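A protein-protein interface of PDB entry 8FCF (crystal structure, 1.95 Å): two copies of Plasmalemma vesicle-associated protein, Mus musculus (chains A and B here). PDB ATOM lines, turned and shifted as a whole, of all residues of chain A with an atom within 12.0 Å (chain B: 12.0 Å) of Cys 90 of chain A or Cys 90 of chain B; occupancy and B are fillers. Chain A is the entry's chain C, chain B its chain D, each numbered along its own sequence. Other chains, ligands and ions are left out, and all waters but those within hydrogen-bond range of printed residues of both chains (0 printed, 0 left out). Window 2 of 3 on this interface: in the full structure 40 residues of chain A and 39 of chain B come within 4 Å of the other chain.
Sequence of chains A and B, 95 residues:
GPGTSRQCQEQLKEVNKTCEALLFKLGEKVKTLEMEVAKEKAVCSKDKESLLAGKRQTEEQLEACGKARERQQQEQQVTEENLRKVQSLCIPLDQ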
ATOM      1  N   GLU A  81      32.312 -17.060  20.908  1.00  0.00           N
ATOM      2  CA  GLU A  81      33.093 -18.266  20.688  1.00  0.00           C
ATOM      3  C   GLU A  81      32.563 -19.400  21.575  1.00  0.00           C
ATOM      4  O   GLU A  81      32.556 -20.556  21.145  1.00  0.00           O
ATOM      5  CB  GLU A  81      34.576 -17.983  20.962  1.00  0.00           C
ATOM      6  CG  GLU A  81      35.526 -19.148  20.737  1.00  0.00           C
ATOM      7  CD  GLU A  81      35.481 -19.819  19.377  1.00  0.00           C
ATOM      8  OE1 GLU A  81      35.161 -19.151  18.366  1.00  0.00           O
ATOM      9  OE2 GLU A  81      35.793 -21.028  19.326  1.00  0.00           O
ATOM     10  N   ASN A  82      32.121 -19.064  22.808  1.00  0.00           N
ATOM     11  CA  ASN A  82      31.545 -20.020  23.748  1.00  0.00           C
ATOM     12  C   ASN A  82      30.254 -20.609  23.190  1.00  0.00           C
ATOM     13  O   ASN A  82      29.997 -21.783  23.437  1.00  0.00           O
ATOM     14  CB  ASN A  82      31.285 -19.363  25.111  1.00  0.00           C
ATOM     15  CG  ASN A  82      32.520 -18.932  25.877  1.00  0.00           C
ATOM     16  OD1 ASN A  82      33.639 -19.388  25.626  1.00  0.00           O
ATOM     17  ND2 ASN A  82      32.331 -18.052  26.865  1.00  0.00           N
ATOM     18  N   LEU A  83      29.440 -19.826  22.443  1.00  0.00           N
ATOM     19  CA  LEU A  83      28.229 -20.355  21.792  1.00  0.00           C
ATOM     20  C   LEU A  83      28.657 -21.406  20.778  1.00  0.00           C
ATOM     21  O   LEU A  83      28.305 -22.561  20.940  1.00  0.00           O
ATOM     22  CB  LEU A  83      27.409 -19.279  21.039  1.00  0.00           C
ATOM     23  CG  LEU A  83      26.265 -18.581  21.753  1.00  0.00           C
ATOM     24  CD1 LEU A  83      25.298 -19.577  22.387  1.00  0.00           C
ATOM     25  CD2 LEU A  83      26.778 -17.554  22.724  1.00  0.00           C
ATOM     26  N   ARG A  84      29.448 -21.014  19.759  1.00  0.00           N
ATOM     27  CA  ARG A  84      29.945 -21.925  18.706  1.00  0.00           C
ATOM     28  C   ARG A  84      30.449 -23.254  19.272  1.00  0.00           C
ATOM     29  O   ARG A  84      30.096 -24.318  18.760  1.00  0.00           O
ATOM     30  CB  ARG A  84      31.090 -21.272  17.912  1.00  0.00           C
ATOM     31  CG  ARG A  84      30.625 -20.279  16.883  1.00  0.00           C
ATOM     32  CD  ARG A  84      31.788 -19.590  16.186  1.00  0.00           C
ATOM     33  NE  ARG A  84      31.523 -18.154  16.022  1.00  0.00           N
ATOM     34  CZ  ARG A  84      32.277 -17.151  16.481  1.00  0.00           C
ATOM     35  NH1 ARG A  84      33.407 -17.400  17.141  1.00  0.00           N
ATOM     36  NH2 ARG A  84      31.921 -15.890  16.257  1.00  0.00           N
ATOM     37  N   LYS A  85      31.259 -23.184  20.337  1.00  0.00           N
ATOM     38  CA  LYS A  85      31.824 -24.370  20.966  1.00  0.00           C
ATOM     39  C   LYS A  85      30.792 -25.193  21.733  1.00  0.00           C
ATOM     40  O   LYS A  85      30.783 -26.410  21.569  1.00  0.00           O
ATOM     41  CB  LYS A  85      33.001 -24.001  21.874  1.00  0.00           C
ATOM     42  CG  LYS A  85      34.229 -23.527  21.095  1.00  0.00           C
ATOM     43  CD  LYS A  85      35.331 -23.064  22.046  1.00  0.00           C
ATOM     44  CE  LYS A  85      36.723 -23.367  21.546  1.00  0.00           C
ATOM     45  NZ  LYS A  85      37.771 -22.712  22.370  1.00  0.00           N
ATOM     46  N   VAL A  86      29.922 -24.572  22.557  1.00  0.00           N
ATOM     47  CA  VAL A  86      28.955 -25.364  23.322  1.00  0.00           C
ATOM     48  C   VAL A  86      27.842 -25.937  22.423  1.00  0.00           C
ATOM     49  O   VAL A  86      27.361 -27.036  22.696  1.00  0.00           O
ATOM     50  CB  VAL A  86      28.388 -24.629  24.576  1.00  0.00           C
ATOM     51  CG1 VAL A  86      27.329 -23.597  24.206  1.00  0.00           C
ATOM     52  CG2 VAL A  86      27.830 -25.636  25.589  1.00  0.00           C
ATOM     53  N   GLN A  87      27.432 -25.216  21.369  1.00  0.00           N
ATOM     54  CA  GLN A  87      26.399 -25.699  20.435  1.00  0.00           C
ATOM     55  C   GLN A  87      26.785 -27.028  19.755  1.00  0.00           C
ATOM     56  O   GLN A  87      25.913 -27.864  19.534  1.00  0.00           O
ATOM     57  CB  GLN A  87      26.029 -24.604  19.415  1.00  0.00           C
ATOM     58  CG  GLN A  87      25.159 -23.527  20.067  1.00  0.00           C
ATOM     59  CD  GLN A  87      24.783 -22.373  19.161  1.00  0.00           C
ATOM     60  OE1 GLN A  87      25.584 -21.904  18.341  1.00  0.00           O
ATOM     61  NE2 GLN A  87      23.550 -21.873  19.294  1.00  0.00           N
ATOM     62  N   SER A  88      28.091 -27.269  19.535  1.00  0.00           N
ATOM     63  CA  SER A  88      28.602 -28.533  18.982  1.00  0.00           C
ATOM     64  C   SER A  88      28.467 -29.752  19.935  1.00  0.00           C
ATOM     65  O   SER A  88      28.679 -30.878  19.476  1.00  0.00           O
ATOM     66  CB  SER A  88      30.063 -28.379  18.554  1.00  0.00           C
ATOM     67  OG  SER A  88      30.981 -28.297  19.636  1.00  0.00           O
ATOM     68  N   LEU A  89      28.158 -29.535  21.246  1.00  0.00           N
ATOM     69  CA  LEU A  89      27.961 -30.604  22.241  1.00  0.00           C
ATOM     70  C   LEU A  89      26.472 -30.897  22.527  1.00  0.00           C
ATOM     71  O   LEU A  89      26.167 -31.947  23.095  1.00  0.00           O
ATOM     72  CB  LEU A  89      28.636 -30.213  23.571  1.00  0.00           C
ATOM     73  CG  LEU A  89      30.091 -29.787  23.510  1.00  0.00           C
ATOM     74  CD1 LEU A  89      30.551 -29.252  24.861  1.00  0.00           C
ATOM     75  CD2 LEU A  89      30.970 -30.939  23.060  1.00  0.00           C
ATOM     76  N   CYS A  90      25.566 -29.950  22.203  1.00  0.00           N
ATOM     77  CA  CYS A  90      24.133 -30.058  22.456  1.00  0.00           C
ATOM     78  C   CYS A  90      23.413 -30.542  21.200  1.00  0.00           C
ATOM     79  O   CYS A  90      22.226 -30.866  21.252  1.00  0.00           O
ATOM     80  CB  CYS A  90      23.574 -28.718  22.939  1.00  0.00           C
ATOM     81  SG  CYS A  90      24.632 -27.836  24.131  1.00  0.00           S
ATOM     82  N   GLU B  81      22.726 -14.195  27.597  1.00  0.00           N
ATOM     83  CA  GLU B  81      21.539 -14.969  27.972  1.00  0.00           C
ATOM     84  C   GLU B  81      21.349 -16.120  26.983  1.00  0.00           C
ATOM     85  O   GLU B  81      20.977 -17.212  27.409  1.00  0.00           O
ATOM     86  CB  GLU B  81      20.265 -14.102  28.040  1.00  0.00           C
ATOM     87  CG  GLU B  81      20.206 -13.066  29.162  1.00  0.00           C
ATOM     88  CD  GLU B  81      21.232 -13.137  30.281  1.00  0.00           C
ATOM     89  OE1 GLU B  81      22.227 -12.377  30.229  1.00  0.00           O
ATOM     90  OE2 GLU B  81      21.031 -13.947  31.216  1.00  0.00           O
ATOM     91  N   ASN B  82      21.640 -15.909  25.680  1.00  0.00           N
ATOM     92  CA  ASN B  82      21.531 -16.992  24.697  1.00  0.00           C
ATOM     93  C   ASN B  82      22.537 -18.116  25.045  1.00  0.00           C
ATOM     94  O   ASN B  82      22.199 -19.291  24.906  1.00  0.00           O
ATOM     95  CB  ASN B  82      21.747 -16.473  23.276  1.00  0.00           C
ATOM     96  CG  ASN B  82      21.409 -17.460  22.179  1.00  0.00           C
ATOM     97  OD1 ASN B  82      20.776 -18.499  22.402  1.00  0.00           O
ATOM     98  ND2 ASN B  82      21.820 -17.150  20.955  1.00  0.00           N
ATOM     99  N   LEU B  83      23.746 -17.748  25.549  1.00  0.00           N
ATOM    100  CA  LEU B  83      24.754 -18.719  25.992  1.00  0.00           C
ATOM    101  C   LEU B  83      24.214 -19.491  27.189  1.00  0.00           C
ATOM    102  O   LEU B  83      24.344 -20.711  27.234  1.00  0.00           O
ATOM    103  CB  LEU B  83      26.089 -18.034  26.361  1.00  0.00           C
ATOM    104  CG  LEU B  83      27.203 -18.936  26.910  1.00  0.00           C
ATOM    105  CD1 LEU B  83      27.525 -20.101  25.962  1.00  0.00           C
ATOM    106  CD2 LEU B  83      28.445 -18.130  27.208  1.00  0.00           C
ATOM    107  N   ARG B  84      23.597 -18.785  28.144  1.00  0.00           N
ATOM    108  CA  ARG B  84      23.013 -19.409  29.327  1.00  0.00           C
ATOM    109  C   ARG B  84      21.868 -20.369  28.930  1.00  0.00           C
ATOM    110  O   ARG B  84      21.874 -21.505  29.367  1.00  0.00           O
ATOM    111  CB  ARG B  84      22.512 -18.331  30.288  1.00  0.00           C
ATOM    112  CG  ARG B  84      22.504 -18.804  31.723  1.00  0.00           C
ATOM    113  CD  ARG B  84      21.154 -18.596  32.359  1.00  0.00           C
ATOM    114  NE  ARG B  84      20.605 -17.306  31.964  1.00  0.00           N
ATOM    115  CZ  ARG B  84      19.371 -17.145  31.509  1.00  0.00           C
ATOM    116  NH1 ARG B  84      18.943 -15.941  31.146  1.00  0.00           N
ATOM    117  NH2 ARG B  84      18.550 -18.185  31.421  1.00  0.00           N
ATOM    118  N   LYS B  85      20.953 -19.937  28.048  1.00  0.00           N
ATOM    119  CA  LYS B  85      19.840 -20.757  27.539  1.00  0.00           C
ATOM    120  C   LYS B  85      20.363 -22.061  26.902  1.00  0.00           C
ATOM    121  O   LYS B  85      19.915 -23.145  27.279  1.00  0.00           O
ATOM    122  CB  LYS B  85      19.016 -19.936  26.508  1.00  0.00           C
ATOM    123  CG  LYS B  85      17.791 -20.654  25.917  1.00  0.00           C
ATOM    124  CD  LYS B  85      18.074 -21.404  24.586  1.00  0.00           C
ATOM    125  CE  LYS B  85      17.549 -22.830  24.578  1.00  0.00           C
ATOM    126  NZ  LYS B  85      18.114 -23.641  23.463  1.00  0.00           N
ATOM    127  N   VAL B  86      21.336 -21.951  25.969  1.00  0.00           N
ATOM    128  CA  VAL B  86      21.928 -23.105  25.275  1.00  0.00           C
ATOM    129  C   VAL B  86      22.608 -24.050  26.268  1.00  0.00           C
ATOM    130  O   VAL B  86      22.413 -25.268  26.165  1.00  0.00           O
ATOM    131  CB  VAL B  86      22.891 -22.672  24.129  1.00  0.00           C
ATOM    132  CG1 VAL B  86      23.693 -23.861  23.600  1.00  0.00           C
ATOM    133  CG2 VAL B  86      22.125 -22.003  22.988  1.00  0.00           C
ATOM    134  N   GLN B  87      23.395 -23.513  27.226  1.00  0.00           N
ATOM    135  CA  GLN B  87      24.064 -24.359  28.235  1.00  0.00           C
ATOM    136  C   GLN B  87      23.089 -24.966  29.238  1.00  0.00           C
ATOM    137  O   GLN B  87      23.295 -26.094  29.684  1.00  0.00           O
ATOM    138  CB  GLN B  87      25.140 -23.568  28.988  1.00  0.00           C
ATOM    139  CG  GLN B  87      26.333 -23.270  28.117  1.00  0.00           C
ATOM    140  CD  GLN B  87      27.542 -22.809  28.882  1.00  0.00           C
ATOM    141  OE1 GLN B  87      27.463 -22.314  30.013  1.00  0.00           O
ATOM    142  NE2 GLN B  87      28.696 -22.953  28.261  1.00  0.00           N
ATOM    143  N   SER B  88      22.059 -24.212  29.628  1.00  0.00           N
ATOM    144  CA  SER B  88      21.048 -24.675  30.580  1.00  0.00           C
ATOM    145  C   SER B  88      20.234 -25.862  29.992  1.00  0.00           C
ATOM    146  O   SER B  88      19.983 -26.831  30.697  1.00  0.00           O
ATOM    147  CB  SER B  88      20.112 -23.526  30.955  1.00  0.00           C
ATOM    148  OG  SER B  88      19.332 -23.836  32.098  1.00  0.00           O
ATOM    149  N   LEU B  89      19.877 -25.796  28.693  1.00  0.00           N
ATOM    150  CA  LEU B  89      19.104 -26.825  27.985  1.00  0.00           C
ATOM    151  C   LEU B  89      19.985 -27.792  27.156  1.00  0.00           C
ATOM    152  O   LEU B  89      19.444 -28.481  26.292  1.00  0.00           O
ATOM    153  CB  LEU B  89      18.064 -26.134  27.054  1.00  0.00           C
ATOM    154  CG  LEU B  89      16.783 -25.578  27.685  1.00  0.00           C
ATOM    155  CD1 LEU B  89      15.840 -26.702  28.116  1.00  0.00           C
ATOM    156  CD2 LEU B  89      17.066 -24.633  28.824  1.00  0.00           C
ATOM    157  N   CYS B  90      21.312 -27.886  27.427  1.00  0.00           N
ATOM    158  CA  CYS B  90      22.219 -28.754  26.653  1.00  0.00           C
ATOM    159  C   CYS B  90      21.937 -30.247  26.855  1.00  0.00           C
ATOM    160  O   CYS B  90      21.632 -30.680  27.962  1.00  0.00           O
ATOM    161  CB  CYS B  90      23.678 -28.422  26.955  1.00  0.00           C
ATOM    162  SG  CYS B  90      24.861 -29.067  25.735  1.00  0.00           S
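The side-chain sulfur (SG) of Cys 90 of chain A is disulfide-bonded to the side-chain sulfur (SG) of Cys 90 of chain B (2.0 Å).
Among the printed residues, merely in contact across the chains: Val 86 of chain A with Val 86 of chain B (3.7 Å), Leu 83 of chain A with Leu 83 of chain B (3.7 Å), Asn 82 of chain A with Leu 83 of chain B (3.7 Å), Val 86 of chain A with Gln 87 of chain B (3.8 Å), Gln 87 of chain A with Val 86 of chain B (3.8 Å), Val 86 of chain A with Leu 83 of chain B (3.9 Å) and Cys 90 of chain A with Val 86 of chain B (3.96 Å).
Printed residues of chain B within 4 Å of Asn 82 of chain A: Leu 83.
Of the printed residues of chain B, Leu 83 of chain A touches Leu 83 (3.7 Å).
Lys 85 of chain A touches none of the printed residues of chain B.
Of the printed residues of chain B, Gln 87 of chain A touches Val 86.
No residue of chain B comes within 4 Å of Ser 88 of chain A.
Of the printed residues of chain B, Cys 90 of chain A touches Val 86 (3.96 Å) and Cys 90 (2.0 Å).
Glu 81 of chain B touches none of the printed residues of chain A.
Of the printed residues of chain A, Leu 83 of chain B touches Asn 82 (3.7 Å), Leu 83 (3.7 Å) and Val 86 (3.9 Å).
Val 86 of chain B touches just these residues of chain A: Val 86 (3.7 Å), Gln 87 (3.8 Å) and Cys 90 (3.96 Å).
No residue of chain A comes within 4 Å of Ser 88 of chain B.
No residue of chain A comes within 4 Å of Leu 89 of chain B.
Of the printed residues of chain A, Cys 90 of chain B touches Cys 90.
The nearest residue of chain B that does not touch Cys 90 of chain A is Leu 89 of chain B (5.3 Å).
The nearest residue of chain A that does not touch Cys 90 of chain B is Leu 89 of chain A (4.03 Å).
Of the 10 printed residues of chain B, 4 touch a printed residue of chain A.
Printed residues of chain B that touch a printed residue of chain A: Leu 83, Val 86, Gln 87 and Cys 90.
Hydrophobic or aromatic side chains of chain B that line the printed part of chain A: Leu 83 and Val 86.
Hydrophobic or aromatic side chains of chain A within 4 Å of the printed part of chain B: Leu 83 and Val 86.
Among the printed residues, 8 pairs touch across the chains.
Leu 83 of chain B touches its own counterpart, Leu 83 of chain A.
Val 86 of chain A touches Leu 83 of chain B, but with the chains exchanged Leu 83 of chain A does not touch Val 86 of chain B (4.04 Å).
Cys 90 of chain A touches Val 86 of chain B, but with the chains exchanged Val 86 of chain A does not touch Cys 90 of chain B (4.4 Å).
Cys 90 of chain B touches its own counterpart, Cys 90 of chain A.
10 positions are printed for both chains.
Of the 8 pairs that touch across the chains among the printed residues, 5 have their exchanged pair printed and touching as well.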
